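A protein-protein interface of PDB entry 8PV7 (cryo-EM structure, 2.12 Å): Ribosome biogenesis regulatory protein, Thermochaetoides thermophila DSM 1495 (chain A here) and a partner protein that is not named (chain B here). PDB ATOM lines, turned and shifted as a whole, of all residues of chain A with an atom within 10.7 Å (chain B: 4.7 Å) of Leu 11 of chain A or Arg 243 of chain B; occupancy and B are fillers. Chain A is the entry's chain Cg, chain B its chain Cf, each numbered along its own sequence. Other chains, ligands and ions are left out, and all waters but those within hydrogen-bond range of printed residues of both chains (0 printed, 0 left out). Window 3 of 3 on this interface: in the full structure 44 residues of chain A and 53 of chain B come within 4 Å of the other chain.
N of Val 244 of chain B lies within hydrogen-bond range of OE1 of Gln 60 of chain A (3.0 Å). NE2 of Gln 60 of chain A sits at hydrogen-bond distance from O of Pro 242 of chain B (3.1 Å). NH1 of Arg 56 of chain A lies close to NH1 of Arg 243 of chain B. NH1 of Arg 243 of chain B lies within hydrogen-bond range of O of Pro 12 of chain A (2.5 Å).
Printed residues of chain B within 4 Å of Pro 12 of chain A: Arg 243. Val 15 of chain A touches none of the printed residues of chain B. Printed residues of chain B within 4 Å of Arg 56 of chain A: Arg 243 and Val 244. Asp 57 of chain A touches none of the printed residues of chain B. Printed residues of chain B within 4 Å of Gln 60 of chain A: Pro 242, Arg 243 and Val 244. Of the printed residues of chain B, Asn 64 of chain A touches Leu 241 (3.4 Å). No residue of chain A comes within 4 Å of Thr 234 of chain B. No residue of chain A comes within 4 Å of Lys 235 of chain B. Of chain A, only Val 13 (3.4 Å) comes within 4 Å of Ser 237 of chain B. Arg 243 of chain B touches five residues of chain A. Val 244 of chain B touches just these residues of chain A: Arg 56, Ala 59 and Gln 60. No residue of chain A comes within 4 Å of Glu 245 of chain B. The nearest residue of chain B that does not touch Leu 11 of chain A is Ser 237 of chain B (4.1 Å). The nearest residue of chain A that does not touch Arg 243 of chain B is Thr 14 of chain A (5.9 Å). The nearest printed residue of chain B that does not touch Ala 59 of chain A is Glu 245 of chain B (6.4 Å).
Printed residues of chain B that touch a printed residue of chain A: Ser 237, Leu 241, Pro 242, Arg 243 and Val 244. Of the 20 printed residues of chain A, 8 touch a printed residue of chain B. Printed residues of chain A that touch a printed residue of chain B: Leu 11, Pro 12, Val 13, Arg 56, Ala 59, Gln 60, Asn 64 and Leu 67. Hydrophobic or aromatic side chains of chain A that line the printed part of chain B: Leu 11, Pro 12, Val 13, Ala 59 and Leu 67.
Arg 243 of chain B touches Leu 11 of chain A. Ser 237 of chain B touches Val 13 of chain A (OG to CG1, 3.4 Å). Val 13 of chain A touches Leu 241 of chain B (CG1 to O, 3.6 Å). Val 13 of chain A touches Pro 242 of chain B. CG1 of Val 13 of chain A touches CA of Arg 243 of chain B, at 3.9 Å. Arg 56 of chain A touches Val 244 of chain B (CD to O, 3.2 Å). CB of Ala 59 of chain A touches CG1 of Val 244 of chain B, 3.9 Å away. Arg 243 of chain B touches Gln 60 of chain A (CA to OE1, 3.96 Å). Asn 64 of chain A touches Leu 241 of chain B (OD1 to CD1, 3.4 Å). Pro 242 of chain B touches Leu 67 of chain A.
O of Gln 60 of chain A lies close to ND2 of Asn 64 of chain A, at 3.2 Å. The guanidinium group of Arg 56 of chain A lies within hydrogen-bond range of the side-chain amide oxygen of Gln 60 of chain A (2.6 Å). The backbone NH (N) of Lys 235 of chain B lies within hydrogen-bond range of the backbone carbonyl oxygen (O) of Arg 243 of chain B. OG of Ser 237 of chain B is in hydrogen-bond range of O of Leu 241 of chain B (2.7 Å). The backbone carbonyl oxygen of Val 13 of chain A lies within hydrogen-bond range of the side-chain amide nitrogen of Asn 64 of chain A, at 2.7 Å. The backbone carbonyl oxygen of Val 13 of chain A lies within hydrogen-bond range of the side-chain amide nitrogen of Gln 60 of chain A, 3.4 Å away.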
ATOM      1  N   LEU A  11      19.493 -16.519  32.262  1.00  0.00           N
ATOM      2  CA  LEU A  11      18.680 -17.695  31.980  1.00  0.00           C
ATOM      3  C   LEU A  11      19.162 -18.373  30.700  1.00  0.00           C
ATOM      4  O   LEU A  11      19.580 -17.698  29.761  1.00  0.00           O
ATOM      5  CB  LEU A  11      17.196 -17.321  31.870  1.00  0.00           C
ATOM      6  CG  LEU A  11      16.518 -16.690  33.091  1.00  0.00           C
ATOM      7  CD1 LEU A  11      16.564 -15.166  33.047  1.00  0.00           C
ATOM      8  CD2 LEU A  11      15.086 -17.183  33.234  1.00  0.00           C
ATOM      9  N   PRO A  12      19.125 -19.704  30.671  1.00  0.00           N
ATOM     10  CA  PRO A  12      19.610 -20.426  29.491  1.00  0.00           C
ATOM     11  C   PRO A  12      18.682 -20.273  28.297  1.00  0.00           C
ATOM     12  O   PRO A  12      17.475 -20.065  28.436  1.00  0.00           O
ATOM     13  CB  PRO A  12      19.660 -21.881  29.969  1.00  0.00           C
ATOM     14  CG  PRO A  12      18.616 -21.950  31.022  1.00  0.00           C
ATOM     15  CD  PRO A  12      18.672 -20.627  31.728  1.00  0.00           C
ATOM     16  N   VAL A  13      19.269 -20.386  27.110  1.00  0.00           N
ATOM     17  CA  VAL A  13      18.530 -20.360  25.859  1.00  0.00           C
ATOM     18  C   VAL A  13      18.537 -21.732  25.191  1.00  0.00           C
ATOM     19  O   VAL A  13      18.212 -21.852  24.013  1.00  0.00           O
ATOM     20  CB  VAL A  13      19.070 -19.280  24.909  1.00  0.00           C
ATOM     21  CG1 VAL A  13      18.809 -17.907  25.475  1.00  0.00           C
ATOM     22  CG2 VAL A  13      20.551 -19.488  24.662  1.00  0.00           C
ATOM     23  N   THR A  14      18.907 -22.770  25.932  1.00  0.00           N
ATOM     24  CA  THR A  14      18.975 -24.122  25.406  1.00  0.00           C
ATOM     25  C   THR A  14      18.072 -25.022  26.236  1.00  0.00           C
ATOM     26  O   THR A  14      17.996 -24.891  27.459  1.00  0.00           O
ATOM     27  CB  THR A  14      20.414 -24.656  25.420  1.00  0.00           C
ATOM     28  OG1 THR A  14      21.302 -23.646  24.928  1.00  0.00           O
ATOM     29  CG2 THR A  14      20.542 -25.884  24.538  1.00  0.00           C
ATOM     30  N   VAL A  15      17.372 -25.922  25.555  1.00  0.00           N
ATOM     31  CA  VAL A  15      16.514 -26.908  26.197  1.00  0.00           C
ATOM     32  C   VAL A  15      17.139 -28.280  26.009  1.00  0.00           C
ATOM     33  O   VAL A  15      17.453 -28.681  24.884  1.00  0.00           O
ATOM     34  CB  VAL A  15      15.080 -26.879  25.630  1.00  0.00           C
ATOM     35  CG1 VAL A  15      14.163 -27.738  26.479  1.00  0.00           C
ATOM     36  CG2 VAL A  15      14.566 -25.451  25.564  1.00  0.00           C
ATOM     37  N   GLU A  16      17.322 -28.997  27.114  1.00  0.00           N
ATOM     38  CA  GLU A  16      17.904 -30.331  27.105  1.00  0.00           C
ATOM     39  C   GLU A  16      16.823 -31.347  27.435  1.00  0.00           C
ATOM     40  O   GLU A  16      16.178 -31.252  28.485  1.00  0.00           O
ATOM     41  CB  GLU A  16      19.059 -30.438  28.106  1.00  0.00           C
ATOM     42  CG  GLU A  16      20.077 -29.311  28.010  1.00  0.00           C
ATOM     43  CD  GLU A  16      20.999 -29.440  26.809  1.00  0.00           C
ATOM     44  OE1 GLU A  16      21.044 -30.527  26.196  1.00  0.00           O
ATOM     45  OE2 GLU A  16      21.683 -28.448  26.480  1.00  0.00           O
ATOM     46  N   GLN A  49       0.776 -23.840  34.501  1.00  0.00           N
ATOM     47  CA  GLN A  49       2.194 -23.515  34.627  1.00  0.00           C
ATOM     48  C   GLN A  49       3.062 -24.573  33.955  1.00  0.00           C
ATOM     49  O   GLN A  49       4.017 -24.240  33.244  1.00  0.00           O
ATOM     50  CB  GLN A  49       2.560 -23.362  36.104  1.00  0.00           C
ATOM     51  CG  GLN A  49       3.629 -22.315  36.409  1.00  0.00           C
ATOM     52  CD  GLN A  49       4.969 -22.611  35.761  1.00  0.00           C
ATOM     53  OE1 GLN A  49       5.775 -23.368  36.300  1.00  0.00           O
ATOM     54  NE2 GLN A  49       5.217 -22.008  34.603  1.00  0.00           N
ATOM     55  N   ALA A  52       2.572 -24.196  30.210  1.00  0.00           N
ATOM     56  CA  ALA A  52       3.293 -23.027  29.727  1.00  0.00           C
ATOM     57  C   ALA A  52       4.791 -23.279  29.694  1.00  0.00           C
ATOM     58  O   ALA A  52       5.493 -22.734  28.841  1.00  0.00           O
ATOM     59  CB  ALA A  52       2.967 -21.815  30.598  1.00  0.00           C
ATOM     60  N   SER A  53       5.302 -24.103  30.612  1.00  0.00           N
ATOM     61  CA  SER A  53       6.711 -24.484  30.552  1.00  0.00           C
ATOM     62  C   SER A  53       7.015 -25.312  29.308  1.00  0.00           C
ATOM     63  O   SER A  53       8.041 -25.098  28.646  1.00  0.00           O
ATOM     64  CB  SER A  53       7.099 -25.255  31.811  1.00  0.00           C
ATOM     65  OG  SER A  53       6.407 -24.756  32.940  1.00  0.00           O
ATOM     66  N   VAL A  54       6.128 -26.255  28.974  1.00  0.00           N
ATOM     67  CA  VAL A  54       6.296 -27.043  27.751  1.00  0.00           C
ATOM     68  C   VAL A  54       6.253 -26.143  26.518  1.00  0.00           C
ATOM     69  O   VAL A  54       7.080 -26.273  25.598  1.00  0.00           O
ATOM     70  CB  VAL A  54       5.228 -28.150  27.685  1.00  0.00           C
ATOM     71  CG1 VAL A  54       5.335 -28.921  26.386  1.00  0.00           C
ATOM     72  CG2 VAL A  54       5.373 -29.087  28.867  1.00  0.00           C
ATOM     73  N   ALA A  55       5.305 -25.203  26.498  1.00  0.00           N
ATOM     74  CA  ALA A  55       5.202 -24.248  25.398  1.00  0.00           C
ATOM     75  C   ALA A  55       6.440 -23.367  25.302  1.00  0.00           C
ATOM     76  O   ALA A  55       6.897 -23.050  24.200  1.00  0.00           O
ATOM     77  CB  ALA A  55       3.958 -23.385  25.579  1.00  0.00           C
ATOM     78  N   ARG A  56       6.986 -22.962  26.449  1.00  0.00           N
ATOM     79  CA  ARG A  56       8.198 -22.152  26.483  1.00  0.00           C
ATOM     80  C   ARG A  56       9.375 -22.895  25.871  1.00  0.00           C
ATOM     81  O   ARG A  56      10.122 -22.326  25.069  1.00  0.00           O
ATOM     82  CB  ARG A  56       8.505 -21.762  27.930  1.00  0.00           C
ATOM     83  CG  ARG A  56       9.080 -20.376  28.145  1.00  0.00           C
ATOM     84  CD  ARG A  56      10.525 -20.281  27.710  1.00  0.00           C
ATOM     85  NE  ARG A  56      11.341 -21.387  28.191  1.00  0.00           N
ATOM     86  CZ  ARG A  56      12.632 -21.522  27.925  1.00  0.00           C
ATOM     87  NH1 ARG A  56      13.285 -20.630  27.202  1.00  0.00           N
ATOM     88  NH2 ARG A  56      13.281 -22.587  28.384  1.00  0.00           N
ATOM     89  N   ASP A  57       9.551 -24.168  26.236  1.00  0.00           N
ATOM     90  CA  ASP A  57      10.653 -24.950  25.677  1.00  0.00           C
ATOM     91  C   ASP A  57      10.497 -25.134  24.171  1.00  0.00           C
ATOM     92  O   ASP A  57      11.470 -24.994  23.412  1.00  0.00           O
ATOM     93  CB  ASP A  57      10.752 -26.308  26.372  1.00  0.00           C
ATOM     94  CG  ASP A  57      10.788 -26.190  27.877  1.00  0.00           C
ATOM     95  OD1 ASP A  57      11.099 -25.092  28.381  1.00  0.00           O
ATOM     96  OD2 ASP A  57      10.497 -27.195  28.559  1.00  0.00           O
ATOM     97  N   GLY A  58       9.275 -25.439  23.720  1.00  0.00           N
ATOM     98  CA  GLY A  58       9.050 -25.617  22.293  1.00  0.00           C
ATOM     99  C   GLY A  58       9.278 -24.345  21.498  1.00  0.00           C
ATOM    100  O   GLY A  58       9.904 -24.371  20.433  1.00  0.00           O
ATOM    101  N   ALA A  59       8.798 -23.213  22.018  1.00  0.00           N
ATOM    102  CA  ALA A  59       9.020 -21.933  21.355  1.00  0.00           C
ATOM    103  C   ALA A  59      10.496 -21.568  21.337  1.00  0.00           C
ATOM    104  O   ALA A  59      10.991 -21.026  20.344  1.00  0.00           O
ATOM    105  CB  ALA A  59       8.206 -20.838  22.040  1.00  0.00           C
ATOM    106  N   GLN A  60      11.215 -21.866  22.424  1.00  0.00           N
ATOM    107  CA  GLN A  60      12.641 -21.562  22.488  1.00  0.00           C
ATOM    108  C   GLN A  60      13.420 -22.339  21.436  1.00  0.00           C
ATOM    109  O   GLN A  60      14.225 -21.759  20.699  1.00  0.00           O
ATOM    110  CB  GLN A  60      13.183 -21.866  23.882  1.00  0.00           C
ATOM    111  CG  GLN A  60      14.671 -21.601  24.038  1.00  0.00           C
ATOM    112  CD  GLN A  60      14.985 -20.136  24.235  1.00  0.00           C
ATOM    113  OE1 GLN A  60      14.502 -19.511  25.175  1.00  0.00           O
ATOM    114  NE2 GLN A  60      15.791 -19.578  23.346  1.00  0.00           N
ATOM    115  N   VAL A  61      13.168 -23.647  21.326  1.00  0.00           N
ATOM    116  CA  VAL A  61      13.932 -24.428  20.354  1.00  0.00           C
ATOM    117  C   VAL A  61      13.515 -24.079  18.930  1.00  0.00           C
ATOM    118  O   VAL A  61      14.339 -24.116  18.009  1.00  0.00           O
ATOM    119  CB  VAL A  61      13.831 -25.942  20.624  1.00  0.00           C
ATOM    120  CG1 VAL A  61      14.519 -26.291  21.925  1.00  0.00           C
ATOM    121  CG2 VAL A  61      12.400 -26.423  20.613  1.00  0.00           C
ATOM    122  N   ILE A  63      12.544 -21.016  17.877  1.00  0.00           N
ATOM    123  CA  ILE A  63      13.193 -19.742  17.577  1.00  0.00           C
ATOM    124  C   ILE A  63      14.687 -19.942  17.349  1.00  0.00           C
ATOM    125  O   ILE A  63      15.274 -19.345  16.438  1.00  0.00           O
ATOM    126  CB  ILE A  63      12.907 -18.725  18.701  1.00  0.00           C
ATOM    127  CG1 ILE A  63      11.436 -18.299  18.677  1.00  0.00           C
ATOM    128  CG2 ILE A  63      13.797 -17.500  18.589  1.00  0.00           C
ATOM    129  CD1 ILE A  63      10.995 -17.675  17.382  1.00  0.00           C
ATOM    130  N   ASN A  64      15.319 -20.804  18.155  1.00  0.00           N
ATOM    131  CA  ASN A  64      16.738 -21.100  17.973  1.00  0.00           C
ATOM    132  C   ASN A  64      17.008 -21.749  16.621  1.00  0.00           C
ATOM    133  O   ASN A  64      17.960 -21.376  15.925  1.00  0.00           O
ATOM    134  CB  ASN A  64      17.233 -22.008  19.096  1.00  0.00           C
ATOM    135  CG  ASN A  64      17.250 -21.320  20.440  1.00  0.00           C
ATOM    136  OD1 ASN A  64      17.245 -20.095  20.523  1.00  0.00           O
ATOM    137  ND2 ASN A  64      17.263 -22.108  21.505  1.00  0.00           N
ATOM    138  N   LEU A  67      16.596 -19.118  13.861  1.00  0.00           N
ATOM    139  CA  LEU A  67      17.658 -18.123  13.826  1.00  0.00           C
ATOM    140  C   LEU A  67      19.021 -18.700  13.479  1.00  0.00           C
ATOM    141  O   LEU A  67      19.901 -17.940  13.065  1.00  0.00           O
ATOM    142  CB  LEU A  67      17.747 -17.395  15.167  1.00  0.00           C
ATOM    143  CG  LEU A  67      16.611 -16.420  15.471  1.00  0.00           C
ATOM    144  CD1 LEU A  67      16.858 -15.721  16.787  1.00  0.00           C
ATOM    145  CD2 LEU A  67      16.456 -15.413  14.349  1.00  0.00           C
ATOM    146  N   ARG B 233       7.411 -13.427  24.025  1.00  0.00           N
ATOM    147  CA  ARG B 233       8.288 -12.313  24.341  1.00  0.00           C
ATOM    148  C   ARG B 233       9.736 -12.771  24.242  1.00  0.00           C
ATOM    149  O   ARG B 233      10.057 -13.931  24.510  1.00  0.00           O
ATOM    150  CB  ARG B 233       8.004 -11.770  25.743  1.00  0.00           C
ATOM    151  CG  ARG B 233       6.968 -10.669  25.780  1.00  0.00           C
ATOM    152  CD  ARG B 233       5.996 -10.856  26.930  1.00  0.00           C
ATOM    153  NE  ARG B 233       6.666 -10.957  28.220  1.00  0.00           N
ATOM    154  CZ  ARG B 233       6.588 -12.012  29.022  1.00  0.00           C
ATOM    155  NH1 ARG B 233       5.869 -13.074  28.698  1.00  0.00           N
ATOM    156  NH2 ARG B 233       7.243 -11.997  30.178  1.00  0.00           N
ATOM    157  N   THR B 234      10.611 -11.855  23.842  1.00  0.00           N
ATOM    158  CA  THR B 234      12.037 -12.124  23.744  1.00  0.00           C
ATOM    159  C   THR B 234      12.799 -11.186  24.667  1.00  0.00           C
ATOM    160  O   THR B 234      12.485  -9.997  24.757  1.00  0.00           O
ATOM    161  CB  THR B 234      12.547 -11.963  22.310  1.00  0.00           C
ATOM    162  OG1 THR B 234      12.222 -10.655  21.825  1.00  0.00           O
ATOM    163  CG2 THR B 234      11.930 -13.008  21.403  1.00  0.00           C
ATOM    164  N   LYS B 235      13.803 -11.730  25.347  1.00  0.00           N
ATOM    165  CA  LYS B 235      14.616 -10.975  26.287  1.00  0.00           C
ATOM    166  C   LYS B 235      16.087 -11.201  25.982  1.00  0.00           C
ATOM    167  O   LYS B 235      16.471 -12.211  25.386  1.00  0.00           O
ATOM    168  CB  LYS B 235      14.319 -11.374  27.737  1.00  0.00           C
ATOM    169  CG  LYS B 235      12.990 -10.877  28.253  1.00  0.00           C
ATOM    170  CD  LYS B 235      12.442 -11.800  29.319  1.00  0.00           C
ATOM    171  CE  LYS B 235      12.735 -11.268  30.708  1.00  0.00           C
ATOM    172  NZ  LYS B 235      12.282 -12.212  31.764  1.00  0.00           N
ATOM    173  N   SER B 237      19.755 -12.292  26.752  1.00  0.00           N
ATOM    174  CA  SER B 237      20.296 -13.374  27.561  1.00  0.00           C
ATOM    175  C   SER B 237      21.815 -13.331  27.654  1.00  0.00           C
ATOM    176  O   SER B 237      22.422 -14.273  28.176  1.00  0.00           O
ATOM    177  CB  SER B 237      19.844 -14.722  26.999  1.00  0.00           C
ATOM    178  OG  SER B 237      20.413 -14.946  25.722  1.00  0.00           O
ATOM    179  N   LEU B 241      21.542 -15.703  20.857  1.00  0.00           N
ATOM    180  CA  LEU B 241      20.160 -16.151  20.844  1.00  0.00           C
ATOM    181  C   LEU B 241      19.371 -15.478  21.966  1.00  0.00           C
ATOM    182  O   LEU B 241      19.848 -15.400  23.102  1.00  0.00           O
ATOM    183  CB  LEU B 241      20.092 -17.667  20.991  1.00  0.00           C
ATOM    184  CG  LEU B 241      20.601 -18.454  19.784  1.00  0.00           C
ATOM    185  CD1 LEU B 241      20.592 -19.943  20.067  1.00  0.00           C
ATOM    186  CD2 LEU B 241      19.779 -18.138  18.550  1.00  0.00           C
ATOM    187  N   PRO B 242      18.172 -14.982  21.682  1.00  0.00           N
ATOM    188  CA  PRO B 242      17.351 -14.368  22.727  1.00  0.00           C
ATOM    189  C   PRO B 242      16.719 -15.404  23.644  1.00  0.00           C
ATOM    190  O   PRO B 242      16.605 -16.585  23.318  1.00  0.00           O
ATOM    191  CB  PRO B 242      16.276 -13.621  21.932  1.00  0.00           C
ATOM    192  CG  PRO B 242      16.147 -14.403  20.681  1.00  0.00           C
ATOM    193  CD  PRO B 242      17.518 -14.926  20.364  1.00  0.00           C
ATOM    194  N   ARG B 243      16.298 -14.929  24.810  1.00  0.00           N
ATOM    195  CA  ARG B 243      15.578 -15.752  25.772  1.00  0.00           C
ATOM    196  C   ARG B 243      14.080 -15.593  25.540  1.00  0.00           C
ATOM    197  O   ARG B 243      13.554 -14.477  25.585  1.00  0.00           O
ATOM    198  CB  ARG B 243      15.948 -15.361  27.200  1.00  0.00           C
ATOM    199  CG  ARG B 243      14.992 -15.887  28.252  1.00  0.00           C
ATOM    200  CD  ARG B 243      15.247 -17.349  28.540  1.00  0.00           C
ATOM    201  NE  ARG B 243      14.300 -17.882  29.509  1.00  0.00           N
ATOM    202  CZ  ARG B 243      14.380 -19.090  30.047  1.00  0.00           C
ATOM    203  NH1 ARG B 243      15.365 -19.918  29.743  1.00  0.00           N
ATOM    204  NH2 ARG B 243      13.451 -19.479  30.914  1.00  0.00           N
ATOM    205  N   VAL B 244      13.401 -16.704  25.300  1.00  0.00           N
ATOM    206  CA  VAL B 244      11.978 -16.694  24.986  1.00  0.00           C
ATOM    207  C   VAL B 244      11.179 -16.722  26.281  1.00  0.00           C
ATOM    208  O   VAL B 244      11.588 -17.347  27.262  1.00  0.00           O
ATOM    209  CB  VAL B 244      11.637 -17.887  24.073  1.00  0.00           C
ATOM    210  CG1 VAL B 244      10.169 -17.906  23.689  1.00  0.00           C
ATOM    211  CG2 VAL B 244      12.509 -17.852  22.834  1.00  0.00           C
ATOM    212  N   GLU B 245      10.068 -15.988  26.314  1.00  0.00           N
ATOM    213  CA  GLU B 245       9.064 -16.130  27.358  1.00  0.00           C
ATOM    214  C   GLU B 245       7.693 -16.181  26.703  1.00  0.00           C
ATOM    215  O   GLU B 245       7.489 -15.617  25.626  1.00  0.00           O
ATOM    216  CB  GLU B 245       9.120 -14.984  28.376  1.00  0.00           C
ATOM    217  CG  GLU B 245      10.405 -14.923  29.187  1.00  0.00           C
ATOM    218  CD  GLU B 245      10.545 -16.067  30.175  1.00  0.00           C
ATOM    219  OE1 GLU B 245       9.519 -16.671  30.552  1.00  0.00           O
ATOM    220  OE2 GLU B 245      11.690 -16.366  30.575  1.00  0.00           O
